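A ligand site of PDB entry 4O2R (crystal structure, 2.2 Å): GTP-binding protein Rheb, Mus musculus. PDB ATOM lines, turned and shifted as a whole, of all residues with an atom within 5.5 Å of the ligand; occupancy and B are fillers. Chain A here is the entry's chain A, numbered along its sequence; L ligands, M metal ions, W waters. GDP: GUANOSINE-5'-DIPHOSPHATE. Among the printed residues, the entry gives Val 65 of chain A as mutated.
Water W2 lies within hydrogen-bond range of O1B of the ligand (2.6 Å), O of Pro 39 (2.8 Å) and NZ of Lys 21 (3.5 Å). Water W1 lies within hydrogen-bond range of an oxygen (O1B) of the ligand and the side-chain hydroxyl of Ser 18.
Merely in contact with the ligand: Tyr 16 (3.8 Å), Arg 17 (3.8 Å), Phe 33 (3.4 Å), Tyr 37 (3.7 Å), Leu 125 (3.5 Å), Ser 151 (3.5 Å) and Lys 153 (3.7 Å). Hydrophobic or aromatic side chains within 4 Å of the ligand: Val 19, Phe 33, Tyr 37, Leu 125 and Ala 152. Of the 26 residues printed, 19 come within 4 Å of the ligand. The nearest printed residue that does not touch the ligand is Val 65 (4.4 Å).
NZ of Lys 21 lies within salt-bridge range of O2B of the ligand. N of Ser 18 sits at hydrogen-bond distance from O1B of the ligand, 2.8 Å away. The backbone NH of Ser 22 lies within hydrogen-bond range of an oxygen (O3B) of the ligand, at 3.0 Å. An oxygen (O4') of the ligand sits at hydrogen-bond distance from the side-chain amino group (NZ) of Lys 122 (3.4 Å). An oxygen (O3') of the ligand is in hydrogen-bond range of the backbone carbonyl oxygen (O) of Asp 35. N of Ser 23 sits at hydrogen-bond distance from O2A of the ligand (2.8 Å). The side-chain carboxylate (OD1) of Asp 124 lies within hydrogen-bond range of a nitrogen (N1) of the ligand (2.7 Å). O3B of the ligand sits at hydrogen-bond distance from OG of Ser 22 (3.1 Å). O6 of the ligand is in hydrogen-bond range of N of Ala 152. N of Val 19 lies within hydrogen-bond range of O2B of the ligand (3.3 Å). ND2 of Asn 121 sits at hydrogen-bond distance from N7 of the ligand, at 3.2 Å. N of Lys 21 sits at hydrogen-bond distance from O2B of the ligand (3.0 Å). An oxygen (O2A) of the ligand is in hydrogen-bond range of the side-chain hydroxyl (OG) of Ser 23, 3.1 Å away. The backbone NH (N) of Gly 20 lies within hydrogen-bond range of an oxygen (O3A) of the ligand, at 3.0 Å. O of Val 34 sits at hydrogen-bond distance from O2' of the ligand, at 3.0 Å.
The side-chain amide nitrogen (ND2) of Asn 121 sits at hydrogen-bond distance from the backbone carbonyl oxygen (O) of Val 19. The side-chain hydroxyl of Ser 150 sits at hydrogen-bond distance from the side-chain amide oxygen of Asn 121 (3.0 Å). O of Ser 18 is in hydrogen-bond range of NZ of Lys 122, at 2.9 Å. The side-chain hydroxyl (OG) of Ser 22 is in hydrogen-bond range of the side-chain carboxylate (OD2) of Asp 62 (2.5 Å). OG of Ser 23 sits at hydrogen-bond distance from O of Val 34 (3.2 Å). The backbone carbonyl oxygen of Tyr 16 lies within hydrogen-bond range of the side-chain amino group of Lys 21 (3.3 Å). The guanidinium group (NH2) of Arg 17 sits at hydrogen-bond distance from the side-chain hydroxyl (OH) of Tyr 16, at 3.2 Å. OG of Ser 151 sits close to N of Lys 153 (3.3 Å).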
ATOM      1  N   TYR A  16      -9.246 -16.401   8.863  1.00  0.00           N
ATOM      2  CA  TYR A  16     -10.428 -15.774   8.234  1.00  0.00           C
ATOM      3  C   TYR A  16     -10.247 -14.276   7.979  1.00  0.00           C
ATOM      4  O   TYR A  16      -9.379 -13.645   8.562  1.00  0.00           O
ATOM      5  CB  TYR A  16     -11.648 -15.976   9.162  1.00  0.00           C
ATOM      6  CG  TYR A  16     -12.983 -15.595   8.575  1.00  0.00           C
ATOM      7  CD1 TYR A  16     -13.482 -16.244   7.462  1.00  0.00           C
ATOM      8  CD2 TYR A  16     -13.763 -14.612   9.167  1.00  0.00           C
ATOM      9  CE1 TYR A  16     -14.718 -15.894   6.909  1.00  0.00           C
ATOM     10  CE2 TYR A  16     -14.995 -14.255   8.634  1.00  0.00           C
ATOM     11  CZ  TYR A  16     -15.463 -14.900   7.504  1.00  0.00           C
ATOM     12  OH  TYR A  16     -16.682 -14.571   6.977  1.00  0.00           O
ATOM     13  N   ARG A  17     -11.096 -13.698   7.128  1.00  0.00           N
ATOM     14  CA  ARG A  17     -11.031 -12.252   6.841  1.00  0.00           C
ATOM     15  C   ARG A  17     -11.280 -11.375   8.073  1.00  0.00           C
ATOM     16  O   ARG A  17     -12.144 -11.690   8.918  1.00  0.00           O
ATOM     17  CB  ARG A  17     -12.006 -11.826   5.738  1.00  0.00           C
ATOM     18  CG  ARG A  17     -13.442 -12.277   5.918  1.00  0.00           C
ATOM     19  CD  ARG A  17     -14.314 -11.728   4.799  1.00  0.00           C
ATOM     20  NE  ARG A  17     -15.532 -12.507   4.625  1.00  0.00           N
ATOM     21  CZ  ARG A  17     -15.620 -13.609   3.886  1.00  0.00           C
ATOM     22  NH1 ARG A  17     -14.546 -14.088   3.261  1.00  0.00           N
ATOM     23  NH2 ARG A  17     -16.785 -14.247   3.771  1.00  0.00           N
ATOM     24  N   SER A  18     -10.501 -10.297   8.138  1.00  0.00           N
ATOM     25  CA  SER A  18     -10.663  -9.260   9.164  1.00  0.00           C
ATOM     26  C   SER A  18     -10.411  -9.721  10.588  1.00  0.00           C
ATOM     27  O   SER A  18     -10.858  -9.069  11.525  1.00  0.00           O
ATOM     28  CB  SER A  18     -12.064  -8.619   9.094  1.00  0.00           C
ATOM     29  OG  SER A  18     -12.263  -7.955   7.857  1.00  0.00           O
ATOM     30  N   VAL A  19      -9.694 -10.825  10.769  1.00  0.00           N
ATOM     31  CA  VAL A  19      -9.358 -11.241  12.129  1.00  0.00           C
ATOM     32  C   VAL A  19      -8.133 -10.470  12.643  1.00  0.00           C
ATOM     33  O   VAL A  19      -7.807 -10.552  13.827  1.00  0.00           O
ATOM     34  CB  VAL A  19      -9.099 -12.753  12.273  1.00  0.00           C
ATOM     35  CG1 VAL A  19     -10.295 -13.564  11.770  1.00  0.00           C
ATOM     36  CG2 VAL A  19      -7.823 -13.167  11.544  1.00  0.00           C
ATOM     37  N   GLY A  20      -7.489  -9.695  11.762  1.00  0.00           N
ATOM     38  CA  GLY A  20      -6.307  -8.928  12.167  1.00  0.00           C
ATOM     39  C   GLY A  20      -4.937  -9.575  11.919  1.00  0.00           C
ATOM     40  O   GLY A  20      -3.952  -9.176  12.547  1.00  0.00           O
ATOM     41  N   LYS A  21      -4.858 -10.544  11.008  1.00  0.00           N
ATOM     42  CA  LYS A  21      -3.574 -11.115  10.591  1.00  0.00           C
ATOM     43  C   LYS A  21      -2.632 -10.003  10.117  1.00  0.00           C
ATOM     44  O   LYS A  21      -1.483  -9.917  10.559  1.00  0.00           O
ATOM     45  CB  LYS A  21      -3.740 -12.158   9.461  1.00  0.00           C
ATOM     46  CG  LYS A  21      -4.885 -13.160   9.635  1.00  0.00           C
ATOM     47  CD  LYS A  21      -5.035 -14.208   8.475  1.00  0.00           C
ATOM     48  CE  LYS A  21      -5.348 -13.676   7.049  1.00  0.00           C
ATOM     49  NZ  LYS A  21      -6.718 -12.983   6.786  1.00  0.00           N
ATOM     50  N   SER A  22      -3.118  -9.152   9.226  1.00  0.00           N
ATOM     51  CA  SER A  22      -2.316  -8.022   8.778  1.00  0.00           C
ATOM     52  C   SER A  22      -1.935  -7.072   9.924  1.00  0.00           C
ATOM     53  O   SER A  22      -0.755  -6.751  10.079  1.00  0.00           O
ATOM     54  CB  SER A  22      -2.999  -7.253   7.656  1.00  0.00           C
ATOM     55  OG  SER A  22      -2.941  -7.985   6.450  1.00  0.00           O
ATOM     56  N   SER A  23      -2.904  -6.646  10.731  1.00  0.00           N
ATOM     57  CA  SER A  23      -2.603  -5.658  11.784  1.00  0.00           C
ATOM     58  C   SER A  23      -1.576  -6.156  12.790  1.00  0.00           C
ATOM     59  O   SER A  23      -0.678  -5.414  13.192  1.00  0.00           O
ATOM     60  CB  SER A  23      -3.877  -5.200  12.498  1.00  0.00           C
ATOM     61  OG  SER A  23      -4.730  -4.526  11.598  1.00  0.00           O
ATOM     62  N   LEU A  24      -1.725  -7.414  13.206  1.00  0.00           N
ATOM     63  CA  LEU A  24      -0.777  -8.053  14.105  1.00  0.00           C
ATOM     64  C   LEU A  24       0.602  -8.065  13.496  1.00  0.00           C
ATOM     65  O   LEU A  24       1.582  -7.760  14.173  1.00  0.00           O
ATOM     66  CB  LEU A  24      -1.175  -9.508  14.366  1.00  0.00           C
ATOM     67  CG  LEU A  24      -2.059  -9.702  15.582  1.00  0.00           C
ATOM     68  CD1 LEU A  24      -2.302 -11.194  15.829  1.00  0.00           C
ATOM     69  CD2 LEU A  24      -1.377  -9.067  16.778  1.00  0.00           C
ATOM     70  N   PHE A  33      -0.339   0.468  14.600  1.00  0.00           N
ATOM     71  CA  PHE A  33      -1.639  -0.158  14.370  1.00  0.00           C
ATOM     72  C   PHE A  33      -2.329   0.483  13.170  1.00  0.00           C
ATOM     73  O   PHE A  33      -2.503   1.687  13.117  1.00  0.00           O
ATOM     74  CB  PHE A  33      -2.531  -0.036  15.616  1.00  0.00           C
ATOM     75  CG  PHE A  33      -3.912  -0.567  15.415  1.00  0.00           C
ATOM     76  CD1 PHE A  33      -4.129  -1.890  15.105  1.00  0.00           C
ATOM     77  CD2 PHE A  33      -5.005   0.276  15.545  1.00  0.00           C
ATOM     78  CE1 PHE A  33      -5.402  -2.383  14.909  1.00  0.00           C
ATOM     79  CE2 PHE A  33      -6.294  -0.204  15.357  1.00  0.00           C
ATOM     80  CZ  PHE A  33      -6.493  -1.534  15.031  1.00  0.00           C
ATOM     81  N   VAL A  34      -2.704  -0.337  12.187  1.00  0.00           N
ATOM     82  CA  VAL A  34      -3.229   0.182  10.923  1.00  0.00           C
ATOM     83  C   VAL A  34      -4.670  -0.264  10.692  1.00  0.00           C
ATOM     84  O   VAL A  34      -5.005  -1.444  10.876  1.00  0.00           O
ATOM     85  CB  VAL A  34      -2.364  -0.265   9.757  1.00  0.00           C
ATOM     86  CG1 VAL A  34      -1.054   0.486   9.773  1.00  0.00           C
ATOM     87  CG2 VAL A  34      -2.134  -1.755   9.846  1.00  0.00           C
ATOM     88  N   ASP A  35      -5.507   0.672  10.273  1.00  0.00           N
ATOM     89  CA  ASP A  35      -6.966   0.485  10.279  1.00  0.00           C
ATOM     90  C   ASP A  35      -7.552  -0.051   8.961  1.00  0.00           C
ATOM     91  O   ASP A  35      -8.785  -0.153   8.818  1.00  0.00           O
ATOM     92  CB  ASP A  35      -7.642   1.802  10.691  1.00  0.00           C
ATOM     93  CG  ASP A  35      -7.153   2.319  12.053  1.00  0.00           C
ATOM     94  OD1 ASP A  35      -6.130   3.055  12.103  1.00  0.00           O
ATOM     95  OD2 ASP A  35      -7.791   1.994  13.077  1.00  0.00           O
ATOM     96  N   SER A  36      -6.670  -0.414   8.027  1.00  0.00           N
ATOM     97  CA  SER A  36      -7.106  -0.881   6.710  1.00  0.00           C
ATOM     98  C   SER A  36      -5.991  -1.658   6.010  1.00  0.00           C
ATOM     99  O   SER A  36      -4.831  -1.301   6.153  1.00  0.00           O
ATOM    100  CB  SER A  36      -7.539   0.311   5.843  1.00  0.00           C
ATOM    101  OG  SER A  36      -8.129  -0.102   4.611  1.00  0.00           O
ATOM    102  N   TYR A  37      -6.356  -2.699   5.239  1.00  0.00           N
ATOM    103  CA  TYR A  37      -5.351  -3.521   4.542  1.00  0.00           C
ATOM    104  C   TYR A  37      -6.012  -4.216   3.337  1.00  0.00           C
ATOM    105  O   TYR A  37      -7.186  -4.584   3.415  1.00  0.00           O
ATOM    106  CB  TYR A  37      -4.604  -4.381   5.551  1.00  0.00           C
ATOM    107  CG  TYR A  37      -3.170  -3.982   5.655  1.00  0.00           C
ATOM    108  CD1 TYR A  37      -2.264  -4.325   4.662  1.00  0.00           C
ATOM    109  CD2 TYR A  37      -2.722  -3.221   6.723  1.00  0.00           C
ATOM    110  CE1 TYR A  37      -0.940  -3.928   4.727  1.00  0.00           C
ATOM    111  CE2 TYR A  37      -1.392  -2.810   6.801  1.00  0.00           C
ATOM    112  CZ  TYR A  37      -0.513  -3.167   5.804  1.00  0.00           C
ATOM    113  OH  TYR A  37       0.813  -2.769   5.882  1.00  0.00           O
ATOM    114  N   PRO A  39      -7.110  -6.977   1.664  1.00  0.00           N
ATOM    115  CA  PRO A  39      -7.279  -8.250   2.380  1.00  0.00           C
ATOM    116  C   PRO A  39      -7.089  -9.500   1.508  1.00  0.00           C
ATOM    117  O   PRO A  39      -6.955 -10.586   2.076  1.00  0.00           O
ATOM    118  CB  PRO A  39      -8.717  -8.168   2.902  1.00  0.00           C
ATOM    119  CG  PRO A  39      -9.415  -7.241   1.953  1.00  0.00           C
ATOM    120  CD  PRO A  39      -8.382  -6.303   1.377  1.00  0.00           C
ATOM    121  N   ASP A  62       2.004 -13.107   5.298  1.00  0.00           N
ATOM    122  CA  ASP A  62       0.710 -12.673   5.765  1.00  0.00           C
ATOM    123  C   ASP A  62      -0.298 -13.054   4.707  1.00  0.00           C
ATOM    124  O   ASP A  62      -0.468 -12.340   3.715  1.00  0.00           O
ATOM    125  CB  ASP A  62       0.726 -11.153   5.937  1.00  0.00           C
ATOM    126  CG  ASP A  62      -0.612 -10.585   6.352  1.00  0.00           C
ATOM    127  OD1 ASP A  62      -1.380 -11.325   7.017  1.00  0.00           O
ATOM    128  OD2 ASP A  62      -0.909  -9.416   6.019  1.00  0.00           O
ATOM    129  N   VAL A  65      -7.084 -13.531   2.629  1.00  0.00           N
ATOM    130  CA  VAL A  65      -8.252 -14.079   3.302  1.00  0.00           C
ATOM    131  C   VAL A  65      -8.478 -15.555   2.987  1.00  0.00           C
ATOM    132  O   VAL A  65      -8.458 -15.967   1.834  1.00  0.00           O
ATOM    133  CB  VAL A  65      -9.506 -13.287   2.908  1.00  0.00           C
ATOM    134  CG1 VAL A  65     -10.750 -14.001   3.368  1.00  0.00           C
ATOM    135  CG2 VAL A  65      -9.430 -11.887   3.479  1.00  0.00           C
ATOM    136  N   ASN A 121      -7.172 -12.934  18.444  1.00  0.00           N
ATOM    137  CA  ASN A 121      -6.839 -11.534  18.366  1.00  0.00           C
ATOM    138  C   ASN A 121      -8.043 -10.647  18.734  1.00  0.00           C
ATOM    139  O   ASN A 121      -9.175 -11.142  18.815  1.00  0.00           O
ATOM    140  CB  ASN A 121      -6.333 -11.213  16.950  1.00  0.00           C
ATOM    141  CG  ASN A 121      -5.764  -9.825  16.830  1.00  0.00           C
ATOM    142  OD1 ASN A 121      -5.065  -9.345  17.733  1.00  0.00           O
ATOM    143  ND2 ASN A 121      -6.067  -9.160  15.723  1.00  0.00           N
ATOM    144  N   LYS A 122      -7.763  -9.369  18.974  1.00  0.00           N
ATOM    145  CA  LYS A 122      -8.754  -8.339  19.301  1.00  0.00           C
ATOM    146  C   LYS A 122      -9.284  -8.450  20.727  1.00  0.00           C
ATOM    147  O   LYS A 122     -10.429  -8.086  20.995  1.00  0.00           O
ATOM    148  CB  LYS A 122      -9.925  -8.343  18.322  1.00  0.00           C
ATOM    149  CG  LYS A 122      -9.550  -8.174  16.846  1.00  0.00           C
ATOM    150  CD  LYS A 122     -10.836  -8.055  16.013  1.00  0.00           C
ATOM    151  CE  LYS A 122     -10.517  -7.957  14.528  1.00  0.00           C
ATOM    152  NZ  LYS A 122     -11.633  -7.348  13.758  1.00  0.00           N
ATOM    153  N   LYS A 123      -8.443  -8.912  21.657  1.00  0.00           N
ATOM    154  CA  LYS A 123      -8.840  -9.001  23.064  1.00  0.00           C
ATOM    155  C   LYS A 123      -9.105  -7.621  23.680  1.00  0.00           C
ATOM    156  O   LYS A 123      -9.615  -7.518  24.785  1.00  0.00           O
ATOM    157  CB  LYS A 123      -7.819  -9.785  23.899  1.00  0.00           C
ATOM    158  CG  LYS A 123      -6.580  -8.970  24.277  1.00  0.00           C
ATOM    159  CD  LYS A 123      -5.532  -9.850  24.946  1.00  0.00           C
ATOM    160  CE  LYS A 123      -4.288  -9.045  25.302  1.00  0.00           C
ATOM    161  NZ  LYS A 123      -4.600  -7.874  26.171  1.00  0.00           N
ATOM    162  N   ASP A 124      -8.784  -6.556  22.957  1.00  0.00           N
ATOM    163  CA  ASP A 124      -9.085  -5.213  23.434  1.00  0.00           C
ATOM    164  C   ASP A 124     -10.565  -4.846  23.272  1.00  0.00           C
ATOM    165  O   ASP A 124     -11.062  -3.911  23.909  1.00  0.00           O
ATOM    166  CB  ASP A 124      -8.205  -4.184  22.717  1.00  0.00           C
ATOM    167  CG  ASP A 124      -8.427  -4.182  21.217  1.00  0.00           C
ATOM    168  OD1 ASP A 124      -7.848  -5.043  20.517  1.00  0.00           O
ATOM    169  OD2 ASP A 124      -9.171  -3.301  20.741  1.00  0.00           O
ATOM    170  N   LEU A 125     -11.271  -5.583  22.419  1.00  0.00           N
ATOM    171  CA  LEU A 125     -12.690  -5.328  22.181  1.00  0.00           C
ATOM    172  C   LEU A 125     -13.559  -6.184  23.089  1.00  0.00           C
ATOM    173  O   LEU A 125     -14.352  -7.000  22.613  1.00  0.00           O
ATOM    174  CB  LEU A 125     -13.045  -5.609  20.721  1.00  0.00           C
ATOM    175  CG  LEU A 125     -12.346  -4.722  19.693  1.00  0.00           C
ATOM    176  CD1 LEU A 125     -12.816  -5.076  18.294  1.00  0.00           C
ATOM    177  CD2 LEU A 125     -12.559  -3.227  20.000  1.00  0.00           C
ATOM    178  N   SER A 150      -4.341 -11.854  21.822  1.00  0.00           N
ATOM    179  CA  SER A 150      -3.576 -10.665  21.449  1.00  0.00           C
ATOM    180  C   SER A 150      -4.458  -9.473  21.106  1.00  0.00           C
ATOM    181  O   SER A 150      -5.674  -9.612  20.933  1.00  0.00           O
ATOM    182  CB  SER A 150      -2.674 -10.961  20.251  1.00  0.00           C
ATOM    183  OG  SER A 150      -3.449 -11.391  19.143  1.00  0.00           O
ATOM    184  N   SER A 151      -3.807  -8.321  21.006  1.00  0.00           N
ATOM    185  CA  SER A 151      -4.399  -7.119  20.445  1.00  0.00           C
ATOM    186  C   SER A 151      -3.386  -6.414  19.580  1.00  0.00           C
ATOM    187  O   SER A 151      -2.320  -6.016  20.058  1.00  0.00           O
ATOM    188  CB  SER A 151      -4.865  -6.158  21.555  1.00  0.00           C
ATOM    189  OG  SER A 151      -5.351  -4.948  20.970  1.00  0.00           O
ATOM    190  N   ALA A 152      -3.711  -6.245  18.311  1.00  0.00           N
ATOM    191  CA  ALA A 152      -2.832  -5.572  17.372  1.00  0.00           C
ATOM    192  C   ALA A 152      -2.566  -4.122  17.756  1.00  0.00           C
ATOM    193  O   ALA A 152      -1.677  -3.493  17.207  1.00  0.00           O
ATOM    194  CB  ALA A 152      -3.399  -5.648  15.976  1.00  0.00           C
ATOM    195  N   LYS A 153      -3.370  -3.583  18.675  1.00  0.00           N
ATOM    196  CA  LYS A 153      -3.131  -2.267  19.259  1.00  0.00           C
ATOM    197  C   LYS A 153      -2.016  -2.264  20.322  1.00  0.00           C
ATOM    198  O   LYS A 153      -1.520  -1.203  20.712  1.00  0.00           O
ATOM    199  CB  LYS A 153      -4.411  -1.713  19.896  1.00  0.00           C
ATOM    200  CG  LYS A 153      -5.487  -1.303  18.909  1.00  0.00           C
ATOM    201  CD  LYS A 153      -6.691  -0.704  19.631  1.00  0.00           C
ATOM    202  CE  LYS A 153      -7.662  -0.015  18.663  1.00  0.00           C
ATOM    203  NZ  LYS A 153      -8.827   0.615  19.353  1.00  0.00           N
HETATM  204  PB  GDP L   1      -6.990  -9.532   8.095  1.00  0.00           P
HETATM  205  O1B GDP L   1      -7.991  -9.753   6.994  1.00  0.00           O
HETATM  206  O2B GDP L   1      -6.920 -10.814   8.910  1.00  0.00           O
HETATM  207  O3B GDP L   1      -5.609  -9.155   7.586  1.00  0.00           O
HETATM  208  O3A GDP L   1      -7.549  -8.366   9.058  1.00  0.00           O
HETATM  209  PA  GDP L   1      -6.869  -6.924   9.247  1.00  0.00           P
HETATM  210  O1A GDP L   1      -6.830  -6.131   7.945  1.00  0.00           O
HETATM  211  O2A GDP L   1      -5.495  -7.041   9.881  1.00  0.00           O
HETATM  212  O5' GDP L   1      -7.923  -6.240  10.261  1.00  0.00           O
HETATM  213  C5' GDP L   1      -9.254  -5.983   9.822  1.00  0.00           C
HETATM  214  C4' GDP L   1      -9.806  -4.816  10.620  1.00  0.00           C
HETATM  215  O4' GDP L   1      -9.760  -5.127  12.014  1.00  0.00           O
HETATM  216  C3' GDP L   1      -8.972  -3.563  10.419  1.00  0.00           C
HETATM  217  O3' GDP L   1      -9.829  -2.415  10.400  1.00  0.00           O
HETATM  218  C2' GDP L   1      -8.112  -3.485  11.661  1.00  0.00           C
HETATM  219  O2' GDP L   1      -7.777  -2.119  11.952  1.00  0.00           O
HETATM  220  C1' GDP L   1      -9.002  -4.128  12.721  1.00  0.00           C
HETATM  221  N9  GDP L   1      -8.208  -4.824  13.755  1.00  0.00           N
HETATM  222  C8  GDP L   1      -7.301  -5.787  13.528  1.00  0.00           C
HETATM  223  N7  GDP L   1      -6.763  -6.238  14.692  1.00  0.00           N
HETATM  224  C5  GDP L   1      -7.347  -5.569  15.684  1.00  0.00           C
HETATM  225  C6  GDP L   1      -7.253  -5.566  17.159  1.00  0.00           C
HETATM  226  O6  GDP L   1      -6.461  -6.334  17.739  1.00  0.00           O
HETATM  227  N1  GDP L   1      -8.027  -4.716  17.850  1.00  0.00           N
HETATM  228  C2  GDP L   1      -8.896  -3.886  17.242  1.00  0.00           C
HETATM  229  N2  GDP L   1      -9.640  -3.066  18.022  1.00  0.00           N
HETATM  230  N3  GDP L   1      -9.044  -3.831  15.892  1.00  0.00           N
HETATM  231  C4  GDP L   1      -8.310  -4.641  15.078  1.00  0.00           C
HETATM  232 MG    MG M   1      -3.891 -10.610   5.779  1.00  0.00          MG
HETATM  233  O   HOH W   1      -9.727  -7.568   5.950  1.00  0.00           O
HETATM  234  O   HOH W   2      -6.552 -10.136   4.809  1.00  0.00           O
HETATM  235  O   HOH W   3     -11.824  -2.564  12.024  1.00  0.00           O
